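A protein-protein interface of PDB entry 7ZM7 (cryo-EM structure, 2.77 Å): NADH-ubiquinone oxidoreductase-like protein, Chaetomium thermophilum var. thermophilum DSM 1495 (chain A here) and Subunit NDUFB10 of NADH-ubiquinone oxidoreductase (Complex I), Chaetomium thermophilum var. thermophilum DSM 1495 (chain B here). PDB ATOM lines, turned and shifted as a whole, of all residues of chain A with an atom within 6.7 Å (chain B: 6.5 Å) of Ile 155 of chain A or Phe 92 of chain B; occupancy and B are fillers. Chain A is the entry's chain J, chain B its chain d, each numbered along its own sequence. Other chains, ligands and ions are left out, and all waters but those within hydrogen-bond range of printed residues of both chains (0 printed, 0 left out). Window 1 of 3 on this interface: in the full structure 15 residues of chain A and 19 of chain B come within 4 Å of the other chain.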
ATOM      1  N   ARG A 152       6.581   1.610  -1.576  1.00  0.00           N
ATOM      2  CA  ARG A 152       6.187   0.233  -1.207  1.00  0.00           C
ATOM      3  C   ARG A 152       7.403  -0.664  -1.219  1.00  0.00           C
ATOM      4  O   ARG A 152       8.348  -0.362  -1.957  1.00  0.00           O
ATOM      5  CB  ARG A 152       5.117  -0.380  -2.107  1.00  0.00           C
ATOM      6  CG  ARG A 152       3.974   0.530  -2.508  1.00  0.00           C
ATOM      7  CD  ARG A 152       3.072  -0.299  -3.401  1.00  0.00           C
ATOM      8  NE  ARG A 152       2.336  -1.324  -2.677  1.00  0.00           N
ATOM      9  CZ  ARG A 152       1.390  -2.085  -3.214  1.00  0.00           C
ATOM     10  NH1 ARG A 152       1.080  -1.944  -4.491  1.00  0.00           N
ATOM     11  NH2 ARG A 152       0.762  -2.987  -2.483  1.00  0.00           N
ATOM     12  N   ARG A 153       7.309  -1.729  -0.434  1.00  0.00           N
ATOM     13  CA  ARG A 153       8.440  -2.661  -0.315  1.00  0.00           C
ATOM     14  C   ARG A 153       7.949  -4.094  -0.542  1.00  0.00           C
ATOM     15  O   ARG A 153       6.746  -4.311  -0.457  1.00  0.00           O
ATOM     16  CB  ARG A 153       9.159  -2.481   1.026  1.00  0.00           C
ATOM     17  CG  ARG A 153       9.976  -1.202   1.124  1.00  0.00           C
ATOM     18  CD  ARG A 153      10.485  -1.011   2.538  1.00  0.00           C
ATOM     19  NE  ARG A 153      11.553  -0.030   2.626  1.00  0.00           N
ATOM     20  CZ  ARG A 153      11.359   1.248   2.916  1.00  0.00           C
ATOM     21  NH1 ARG A 153      12.381   2.080   2.969  1.00  0.00           N
ATOM     22  NH2 ARG A 153      10.135   1.689   3.138  1.00  0.00           N
ATOM     23  N   PRO A 154       8.829  -5.079  -0.844  1.00  0.00           N
ATOM     24  CA  PRO A 154       8.410  -6.460  -0.984  1.00  0.00           C
ATOM     25  C   PRO A 154       8.014  -6.966   0.410  1.00  0.00           C
ATOM     26  O   PRO A 154       8.704  -6.700   1.370  1.00  0.00           O
ATOM     27  CB  PRO A 154       9.695  -7.155  -1.437  1.00  0.00           C
ATOM     28  CG  PRO A 154      10.818  -6.270  -0.975  1.00  0.00           C
ATOM     29  CD  PRO A 154      10.258  -4.871  -1.068  1.00  0.00           C
ATOM     30  N   ILE A 155       6.875  -7.667   0.479  1.00  0.00           N
ATOM     31  CA  ILE A 155       6.377  -8.124   1.770  1.00  0.00           C
ATOM     32  C   ILE A 155       7.461  -8.879   2.528  1.00  0.00           C
ATOM     33  O   ILE A 155       7.558  -8.785   3.754  1.00  0.00           O
ATOM     34  CB  ILE A 155       5.114  -8.979   1.562  1.00  0.00           C
ATOM     35  CG1 ILE A 155       4.407  -9.203   2.881  1.00  0.00           C
ATOM     36  CG2 ILE A 155       5.426 -10.297   0.868  1.00  0.00           C
ATOM     37  CD1 ILE A 155       3.892  -7.975   3.408  1.00  0.00           C
ATOM     38  N   GLU A 156       8.276  -9.660   1.825  1.00  0.00           N
ATOM     39  CA  GLU A 156       9.325 -10.491   2.485  1.00  0.00           C
ATOM     40  C   GLU A 156      10.328  -9.595   3.200  1.00  0.00           C
ATOM     41  O   GLU A 156      10.801  -9.987   4.270  1.00  0.00           O
ATOM     42  CB  GLU A 156      10.099 -11.294   1.437  1.00  0.00           C
ATOM     43  CG  GLU A 156       9.230 -12.218   0.601  1.00  0.00           C
ATOM     44  CD  GLU A 156       8.534 -11.579  -0.591  1.00  0.00           C
ATOM     45  OE1 GLU A 156       8.744 -10.371  -0.825  1.00  0.00           O
ATOM     46  OE2 GLU A 156       7.779 -12.292  -1.282  1.00  0.00           O
ATOM     47  N   GLU A 157      10.620  -8.437   2.622  1.00  0.00           N
ATOM     48  CA  GLU A 157      11.627  -7.523   3.200  1.00  0.00           C
ATOM     49  C   GLU A 157      11.184  -7.051   4.585  1.00  0.00           C
ATOM     50  O   GLU A 157      12.005  -7.115   5.515  1.00  0.00           O
ATOM     51  CB  GLU A 157      11.763  -6.325   2.261  1.00  0.00           C
ATOM     52  CG  GLU A 157      12.608  -5.201   2.833  1.00  0.00           C
ATOM     53  CD  GLU A 157      12.686  -3.959   1.966  1.00  0.00           C
ATOM     54  OE1 GLU A 157      12.478  -4.082   0.743  1.00  0.00           O
ATOM     55  OE2 GLU A 157      12.945  -2.872   2.515  1.00  0.00           O
ATOM     56  N   THR A 158       9.945  -6.574   4.706  1.00  0.00           N
ATOM     57  CA  THR A 158       9.449  -6.058   6.005  1.00  0.00           C
ATOM     58  C   THR A 158       9.384  -7.204   7.008  1.00  0.00           C
ATOM     59  O   THR A 158       9.807  -6.995   8.157  1.00  0.00           O
ATOM     60  CB  THR A 158       8.064  -5.427   5.860  1.00  0.00           C
ATOM     61  OG1 THR A 158       8.150  -4.450   4.824  1.00  0.00           O
ATOM     62  CG2 THR A 158       7.559  -4.790   7.136  1.00  0.00           C
ATOM     63  N   LEU A 159       8.975  -8.391   6.569  1.00  0.00           N
ATOM     64  CA  LEU A 159       8.770  -9.500   7.532  1.00  0.00           C
ATOM     65  C   LEU A 159      10.081  -9.798   8.247  1.00  0.00           C
ATOM     66  O   LEU A 159      10.032 -10.200   9.402  1.00  0.00           O
ATOM     67  CB  LEU A 159       8.229 -10.731   6.808  1.00  0.00           C
ATOM     68  CG  LEU A 159       6.765 -10.620   6.384  1.00  0.00           C
ATOM     69  CD1 LEU A 159       6.292 -11.888   5.694  1.00  0.00           C
ATOM     70  CD2 LEU A 159       5.878 -10.283   7.570  1.00  0.00           C
ATOM     71  N   ALA A 160      11.218  -9.652   7.578  1.00  0.00           N
ATOM     72  CA  ALA A 160      12.459 -10.044   8.267  1.00  0.00           C
ATOM     73  C   ALA A 160      12.657  -9.192   9.525  1.00  0.00           C
ATOM     74  O   ALA A 160      12.964  -9.777  10.580  1.00  0.00           O
ATOM     75  CB  ALA A 160      13.619  -9.881   7.322  1.00  0.00           C
ATOM     76  N   ILE A 162      10.425  -7.249  11.326  1.00  0.00           N
ATOM     77  CA  ILE A 162       9.367  -7.323  12.373  1.00  0.00           C
ATOM     78  C   ILE A 162       8.958  -8.769  12.646  1.00  0.00           C
ATOM     79  O   ILE A 162       8.733  -9.095  13.823  1.00  0.00           O
ATOM     80  CB  ILE A 162       8.166  -6.418  12.043  1.00  0.00           C
ATOM     81  CG1 ILE A 162       7.566  -6.702  10.664  1.00  0.00           C
ATOM     82  CG2 ILE A 162       8.548  -4.957  12.207  1.00  0.00           C
ATOM     83  CD1 ILE A 162       6.205  -6.087  10.458  1.00  0.00           C
ATOM     84  N   ILE A 168       0.467  -9.045  12.583  1.00  0.00           N
ATOM     85  CA  ILE A 168       0.892  -9.072  11.165  1.00  0.00           C
ATOM     86  C   ILE A 168       0.684 -10.518  10.740  1.00  0.00           C
ATOM     87  O   ILE A 168       1.594 -11.320  10.940  1.00  0.00           O
ATOM     88  CB  ILE A 168       2.354  -8.620  11.015  1.00  0.00           C
ATOM     89  CG1 ILE A 168       2.630  -7.321  11.774  1.00  0.00           C
ATOM     90  CG2 ILE A 168       2.742  -8.514   9.548  1.00  0.00           C
ATOM     91  CD1 ILE A 168       1.989  -6.103  11.160  1.00  0.00           C
ATOM     92  N   PRO A 170       0.302 -12.500   7.578  1.00  0.00           N
ATOM     93  CA  PRO A 170       0.384 -12.419   6.121  1.00  0.00           C
ATOM     94  C   PRO A 170      -0.382 -13.592   5.510  1.00  0.00           C
ATOM     95  O   PRO A 170      -0.619 -14.545   6.207  1.00  0.00           O
ATOM     96  CB  PRO A 170       1.893 -12.437   5.835  1.00  0.00           C
ATOM     97  CG  PRO A 170       2.529 -12.203   7.183  1.00  0.00           C
ATOM     98  CD  PRO A 170       1.585 -12.856   8.165  1.00  0.00           C
ATOM     99  N   PRO A 171      -0.795 -13.535   4.233  1.00  0.00           N
ATOM    100  CA  PRO A 171      -1.616 -14.611   3.687  1.00  0.00           C
ATOM    101  C   PRO A 171      -0.876 -15.940   3.863  1.00  0.00           C
ATOM    102  O   PRO A 171       0.272 -16.015   3.494  1.00  0.00           O
ATOM    103  CB  PRO A 171      -1.736 -14.206   2.218  1.00  0.00           C
ATOM    104  CG  PRO A 171      -1.574 -12.703   2.224  1.00  0.00           C
ATOM    105  CD  PRO A 171      -0.531 -12.450   3.289  1.00  0.00           C
ATOM    106  N   LYS B  88      -7.887  -3.611  10.480  1.00  0.00           N
ATOM    107  CA  LYS B  88      -6.410  -3.575  10.614  1.00  0.00           C
ATOM    108  C   LYS B  88      -5.813  -2.354   9.927  1.00  0.00           C
ATOM    109  O   LYS B  88      -4.619  -2.148  10.070  1.00  0.00           O
ATOM    110  CB  LYS B  88      -5.837  -4.911  10.138  1.00  0.00           C
ATOM    111  CG  LYS B  88      -6.248  -6.124  10.957  1.00  0.00           C
ATOM    112  CD  LYS B  88      -5.710  -6.095  12.368  1.00  0.00           C
ATOM    113  CE  LYS B  88      -4.201  -6.021  12.416  1.00  0.00           C
ATOM    114  NZ  LYS B  88      -3.692  -5.952  13.805  1.00  0.00           N
ATOM    115  N   GLY B  89      -6.630  -1.563   9.255  1.00  0.00           N
ATOM    116  CA  GLY B  89      -6.142  -0.379   8.534  1.00  0.00           C
ATOM    117  C   GLY B  89      -5.618  -0.696   7.147  1.00  0.00           C
ATOM    118  O   GLY B  89      -5.834  -1.822   6.680  1.00  0.00           O
ATOM    119  N   TYR B  90      -4.960   0.272   6.506  1.00  0.00           N
ATOM    120  CA  TYR B  90      -4.397   0.105   5.177  1.00  0.00           C
ATOM    121  C   TYR B  90      -2.889   0.265   5.169  1.00  0.00           C
ATOM    122  O   TYR B  90      -2.254  -0.004   4.151  1.00  0.00           O
ATOM    123  CB  TYR B  90      -5.019   1.121   4.214  1.00  0.00           C
ATOM    124  CG  TYR B  90      -4.789   2.565   4.594  1.00  0.00           C
ATOM    125  CD1 TYR B  90      -3.566   3.177   4.378  1.00  0.00           C
ATOM    126  CD2 TYR B  90      -5.799   3.321   5.152  1.00  0.00           C
ATOM    127  CE1 TYR B  90      -3.359   4.478   4.724  1.00  0.00           C
ATOM    128  CE2 TYR B  90      -5.595   4.627   5.493  1.00  0.00           C
ATOM    129  CZ  TYR B  90      -4.378   5.199   5.271  1.00  0.00           C
ATOM    130  OH  TYR B  90      -4.165   6.508   5.611  1.00  0.00           O
ATOM    131  N   LEU B  91      -2.310   0.697   6.279  1.00  0.00           N
ATOM    132  CA  LEU B  91      -0.941   1.179   6.279  1.00  0.00           C
ATOM    133  C   LEU B  91       0.021   0.078   5.902  1.00  0.00           C
ATOM    134  O   LEU B  91       1.012   0.316   5.207  1.00  0.00           O
ATOM    135  CB  LEU B  91      -0.604   1.730   7.656  1.00  0.00           C
ATOM    136  CG  LEU B  91       0.676   2.520   7.806  1.00  0.00           C
ATOM    137  CD1 LEU B  91       0.565   3.761   6.964  1.00  0.00           C
ATOM    138  CD2 LEU B  91       0.855   2.850   9.257  1.00  0.00           C
ATOM    139  N   PHE B  92      -0.249  -1.135   6.362  1.00  0.00           N
ATOM    140  CA  PHE B  92       0.559  -2.266   5.955  1.00  0.00           C
ATOM    141  C   PHE B  92       0.413  -2.550   4.466  1.00  0.00           C
ATOM    142  O   PHE B  92       1.409  -2.767   3.775  1.00  0.00           O
ATOM    143  CB  PHE B  92       0.182  -3.488   6.781  1.00  0.00           C
ATOM    144  CG  PHE B  92       1.182  -4.564   6.696  1.00  0.00           C
ATOM    145  CD1 PHE B  92       1.128  -5.470   5.674  1.00  0.00           C
ATOM    146  CD2 PHE B  92       2.223  -4.623   7.582  1.00  0.00           C
ATOM    147  CE1 PHE B  92       2.054  -6.425   5.563  1.00  0.00           C
ATOM    148  CE2 PHE B  92       3.164  -5.584   7.471  1.00  0.00           C
ATOM    149  CZ  PHE B  92       3.079  -6.490   6.461  1.00  0.00           C
ATOM    150  N   GLU B  93      -0.818  -2.550   3.958  1.00  0.00           N
ATOM    151  CA  GLU B  93      -1.049  -2.880   2.524  1.00  0.00           C
ATOM    152  C   GLU B  93      -0.516  -1.760   1.624  1.00  0.00           C
ATOM    153  O   GLU B  93      -0.140  -2.072   0.487  1.00  0.00           O
ATOM    154  CB  GLU B  93      -2.527  -3.145   2.246  1.00  0.00           C
ATOM    155  CG  GLU B  93      -2.937  -4.596   2.397  1.00  0.00           C
ATOM    156  CD  GLU B  93      -4.221  -4.926   1.656  1.00  0.00           C
ATOM    157  OE1 GLU B  93      -4.225  -4.823   0.413  1.00  0.00           O
ATOM    158  OE2 GLU B  93      -5.217  -5.268   2.323  1.00  0.00           O
ATOM    159  N   GLN B  94      -0.509  -0.512   2.105  1.00  0.00           N
ATOM    160  CA  GLN B  94      -0.005   0.593   1.297  1.00  0.00           C
ATOM    161  C   GLN B  94       1.495   0.500   1.102  1.00  0.00           C
ATOM    162  O   GLN B  94       2.009   0.874   0.049  1.00  0.00           O
ATOM    163  CB  GLN B  94      -0.368   1.928   1.938  1.00  0.00           C
ATOM    164  CG  GLN B  94      -0.176   3.105   1.022  1.00  0.00           C
ATOM    165  CD  GLN B  94      -0.653   4.388   1.617  1.00  0.00           C
ATOM    166  OE1 GLN B  94      -1.832   4.697   1.571  1.00  0.00           O
ATOM    167  NE2 GLN B  94       0.259   5.160   2.170  1.00  0.00           N
ATOM    168  N   GLN B  95       2.208   0.005   2.105  1.00  0.00           N
ATOM    169  CA  GLN B  95       3.658   0.038   2.139  1.00  0.00           C
ATOM    170  C   GLN B  95       4.306  -1.273   1.760  1.00  0.00           C
ATOM    171  O   GLN B  95       5.533  -1.355   1.783  1.00  0.00           O
ATOM    172  CB  GLN B  95       4.139   0.413   3.525  1.00  0.00           C
ATOM    173  CG  GLN B  95       3.732   1.754   4.006  1.00  0.00           C
ATOM    174  CD  GLN B  95       4.152   1.951   5.419  1.00  0.00           C
ATOM    175  OE1 GLN B  95       4.786   1.082   6.004  1.00  0.00           O
ATOM    176  NE2 GLN B  95       3.798   3.083   5.991  1.00  0.00           N
ATOM    177  N   ASN B  96       3.529  -2.300   1.449  1.00  0.00           N
ATOM    178  CA  ASN B  96       4.053  -3.597   1.052  1.00  0.00           C
ATOM    179  C   ASN B  96       3.285  -4.057  -0.169  1.00  0.00           C
ATOM    180  O   ASN B  96       2.070  -3.872  -0.236  1.00  0.00           O
ATOM    181  CB  ASN B  96       3.908  -4.628   2.170  1.00  0.00           C
ATOM    182  CG  ASN B  96       4.645  -4.243   3.424  1.00  0.00           C
ATOM    183  OD1 ASN B  96       5.808  -4.587   3.603  1.00  0.00           O
ATOM    184  ND2 ASN B  96       3.968  -3.541   4.312  1.00  0.00           N
ATOM    185  N   TYR B  97       3.975  -4.638  -1.138  1.00  0.00           N
ATOM    186  CA  TYR B  97       3.312  -5.363  -2.217  1.00  0.00           C
ATOM    187  C   TYR B  97       3.527  -6.856  -2.043  1.00  0.00           C
ATOM    188  O   TYR B  97       4.644  -7.309  -1.798  1.00  0.00           O
ATOM    189  CB  TYR B  97       3.766  -4.880  -3.600  1.00  0.00           C
ATOM    190  CG  TYR B  97       5.216  -5.073  -3.916  1.00  0.00           C
ATOM    191  CD1 TYR B  97       5.684  -6.245  -4.485  1.00  0.00           C
ATOM    192  CD2 TYR B  97       6.132  -4.084  -3.612  1.00  0.00           C
ATOM    193  CE1 TYR B  97       7.026  -6.417  -4.756  1.00  0.00           C
ATOM    194  CE2 TYR B  97       7.473  -4.241  -3.887  1.00  0.00           C
ATOM    195  CZ  TYR B  97       7.916  -5.410  -4.452  1.00  0.00           C
ATOM    196  OH  TYR B  97       9.254  -5.564  -4.722  1.00  0.00           O
ATOM    197  N   TRP B  98       2.433  -7.598  -2.100  1.00  0.00           N
ATOM    198  CA  TRP B  98       2.418  -9.044  -1.968  1.00  0.00           C
ATOM    199  C   TRP B  98       1.661  -9.632  -3.142  1.00  0.00           C
ATOM    200  O   TRP B  98       0.674  -9.054  -3.603  1.00  0.00           O
ATOM    201  CB  TRP B  98       1.755  -9.482  -0.668  1.00  0.00           C
ATOM    202  CG  TRP B  98       1.554 -10.957  -0.583  1.00  0.00           C
ATOM    203  CD1 TRP B  98       2.417 -11.872  -0.076  1.00  0.00           C
ATOM    204  CD2 TRP B  98       0.417 -11.684  -1.026  1.00  0.00           C
ATOM    205  NE1 TRP B  98       1.889 -13.127  -0.178  1.00  0.00           N
ATOM    206  CE2 TRP B  98       0.658 -13.037  -0.761  1.00  0.00           C
ATOM    207  CE3 TRP B  98      -0.786 -11.323  -1.631  1.00  0.00           C
ATOM    208  CZ2 TRP B  98      -0.253 -14.023  -1.072  1.00  0.00           C
ATOM    209  CZ3 TRP B  98      -1.687 -12.298  -1.930  1.00  0.00           C
ATOM    210  CH2 TRP B  98      -1.421 -13.633  -1.653  1.00  0.00           C
ATOM    211  N   SER B  99       2.114 -10.786  -3.617  1.00  0.00           N
ATOM    212  CA  SER B  99       1.504 -11.435  -4.764  1.00  0.00           C
ATOM    213  C   SER B  99       1.254 -12.900  -4.451  1.00  0.00           C
ATOM    214  O   SER B  99       1.855 -13.475  -3.542  1.00  0.00           O
ATOM    215  CB  SER B  99       2.382 -11.304  -6.013  1.00  0.00           C
ATOM    216  OG  SER B  99       1.770 -11.928  -7.126  1.00  0.00           O
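The backbone carbonyl oxygen of Tyr 97 of chain B sits at hydrogen-bond distance from the backbone NH of Ile 155 of chain A (3.2 Å). The backbone NH of Arg 153 of chain A sits at hydrogen-bond distance from the backbone carbonyl oxygen of Gln 95 of chain B, at 2.9 Å. The side-chain hydroxyl of Thr 158 of chain A is in hydrogen-bond range of the side-chain amide oxygen of Asn 96 of chain B. The guanidinium group (NH2) of Arg 152 of chain A is in hydrogen-bond range of the backbone carbonyl oxygen (O) of Glu 93 of chain B, 3.2 Å away. The guanidinium group of Arg 152 of chain A sits at hydrogen-bond distance from the backbone carbonyl oxygen of Asn 96 of chain B (2.7 Å). N of Tyr 97 of chain B sits at hydrogen-bond distance from O of Arg 153 of chain A (2.9 Å).
O of Phe 92 of chain B is in hydrogen-bond range of ND2 of Asn 96 of chain B (2.7 Å). NE of Arg 153 of chain A lies within salt-bridge range of OE2 of Glu 157 of chain A.
Among the printed residues, merely in contact across the chains: Arg 153 of chain A with Asn 96 of chain B (3.2 Å), Ile 155 of chain A with Phe 92 of chain B (3.2 Å), Arg 152 of chain A with Gln 94 of chain B (3.2 Å), Pro 154 of chain A with Tyr 97 of chain B (3.4 Å), Arg 152 of chain A with Gln 95 of chain B (3.4 Å), Arg 152 of chain A with Tyr 97 of chain B (3.5 Å), Ile 155 of chain A with Trp 98 of chain B (3.5 Å), Ile 155 of chain A with Asn 96 of chain B (3.6 Å), Pro 171 of chain A with Trp 98 of chain B (3.6 Å) and Ile 168 of chain A with Phe 92 of chain B (3.6 Å).
Of chain B, only Phe 92, Asn 96, Tyr 97 and Trp 98 come within 4 Å of Ile 155 of chain A. Glu 157 of chain A touches none of the printed residues of chain B. Printed residues of chain A within 4 Å of Phe 92 of chain B: Ile 155 and Ile 168. Printed residues of chain A within 4 Å of Glu 93 of chain B: Arg 152 (3.2 Å). Printed residues of chain A within 4 Å of Gln 94 of chain B: Arg 152. Printed residues of chain A within 4 Å of Tyr 97 of chain B: Arg 152 (3.5 Å), Arg 153 (2.9 Å), Pro 154 (3.4 Å) and Ile 155 (3.2 Å). The nearest printed residue of chain A that does not touch Glu 93 of chain B is Ile 155 of chain A (7.2 Å).
Of the 12 printed residues of chain B, 7 touch a printed residue of chain A. Hydrophobic or aromatic side chains of chain B that line the printed part of chain A: Phe 92, Tyr 97 and Trp 98. Hydrophobic or aromatic side chains of chain A that line the printed part of chain B: Pro 154, Ile 155, Ile 168 and Pro 171. Among the printed residues, no Asp or Glu carboxylate lies within 4 Å of a Lys or Arg side-chain nitrogen of the other chain.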
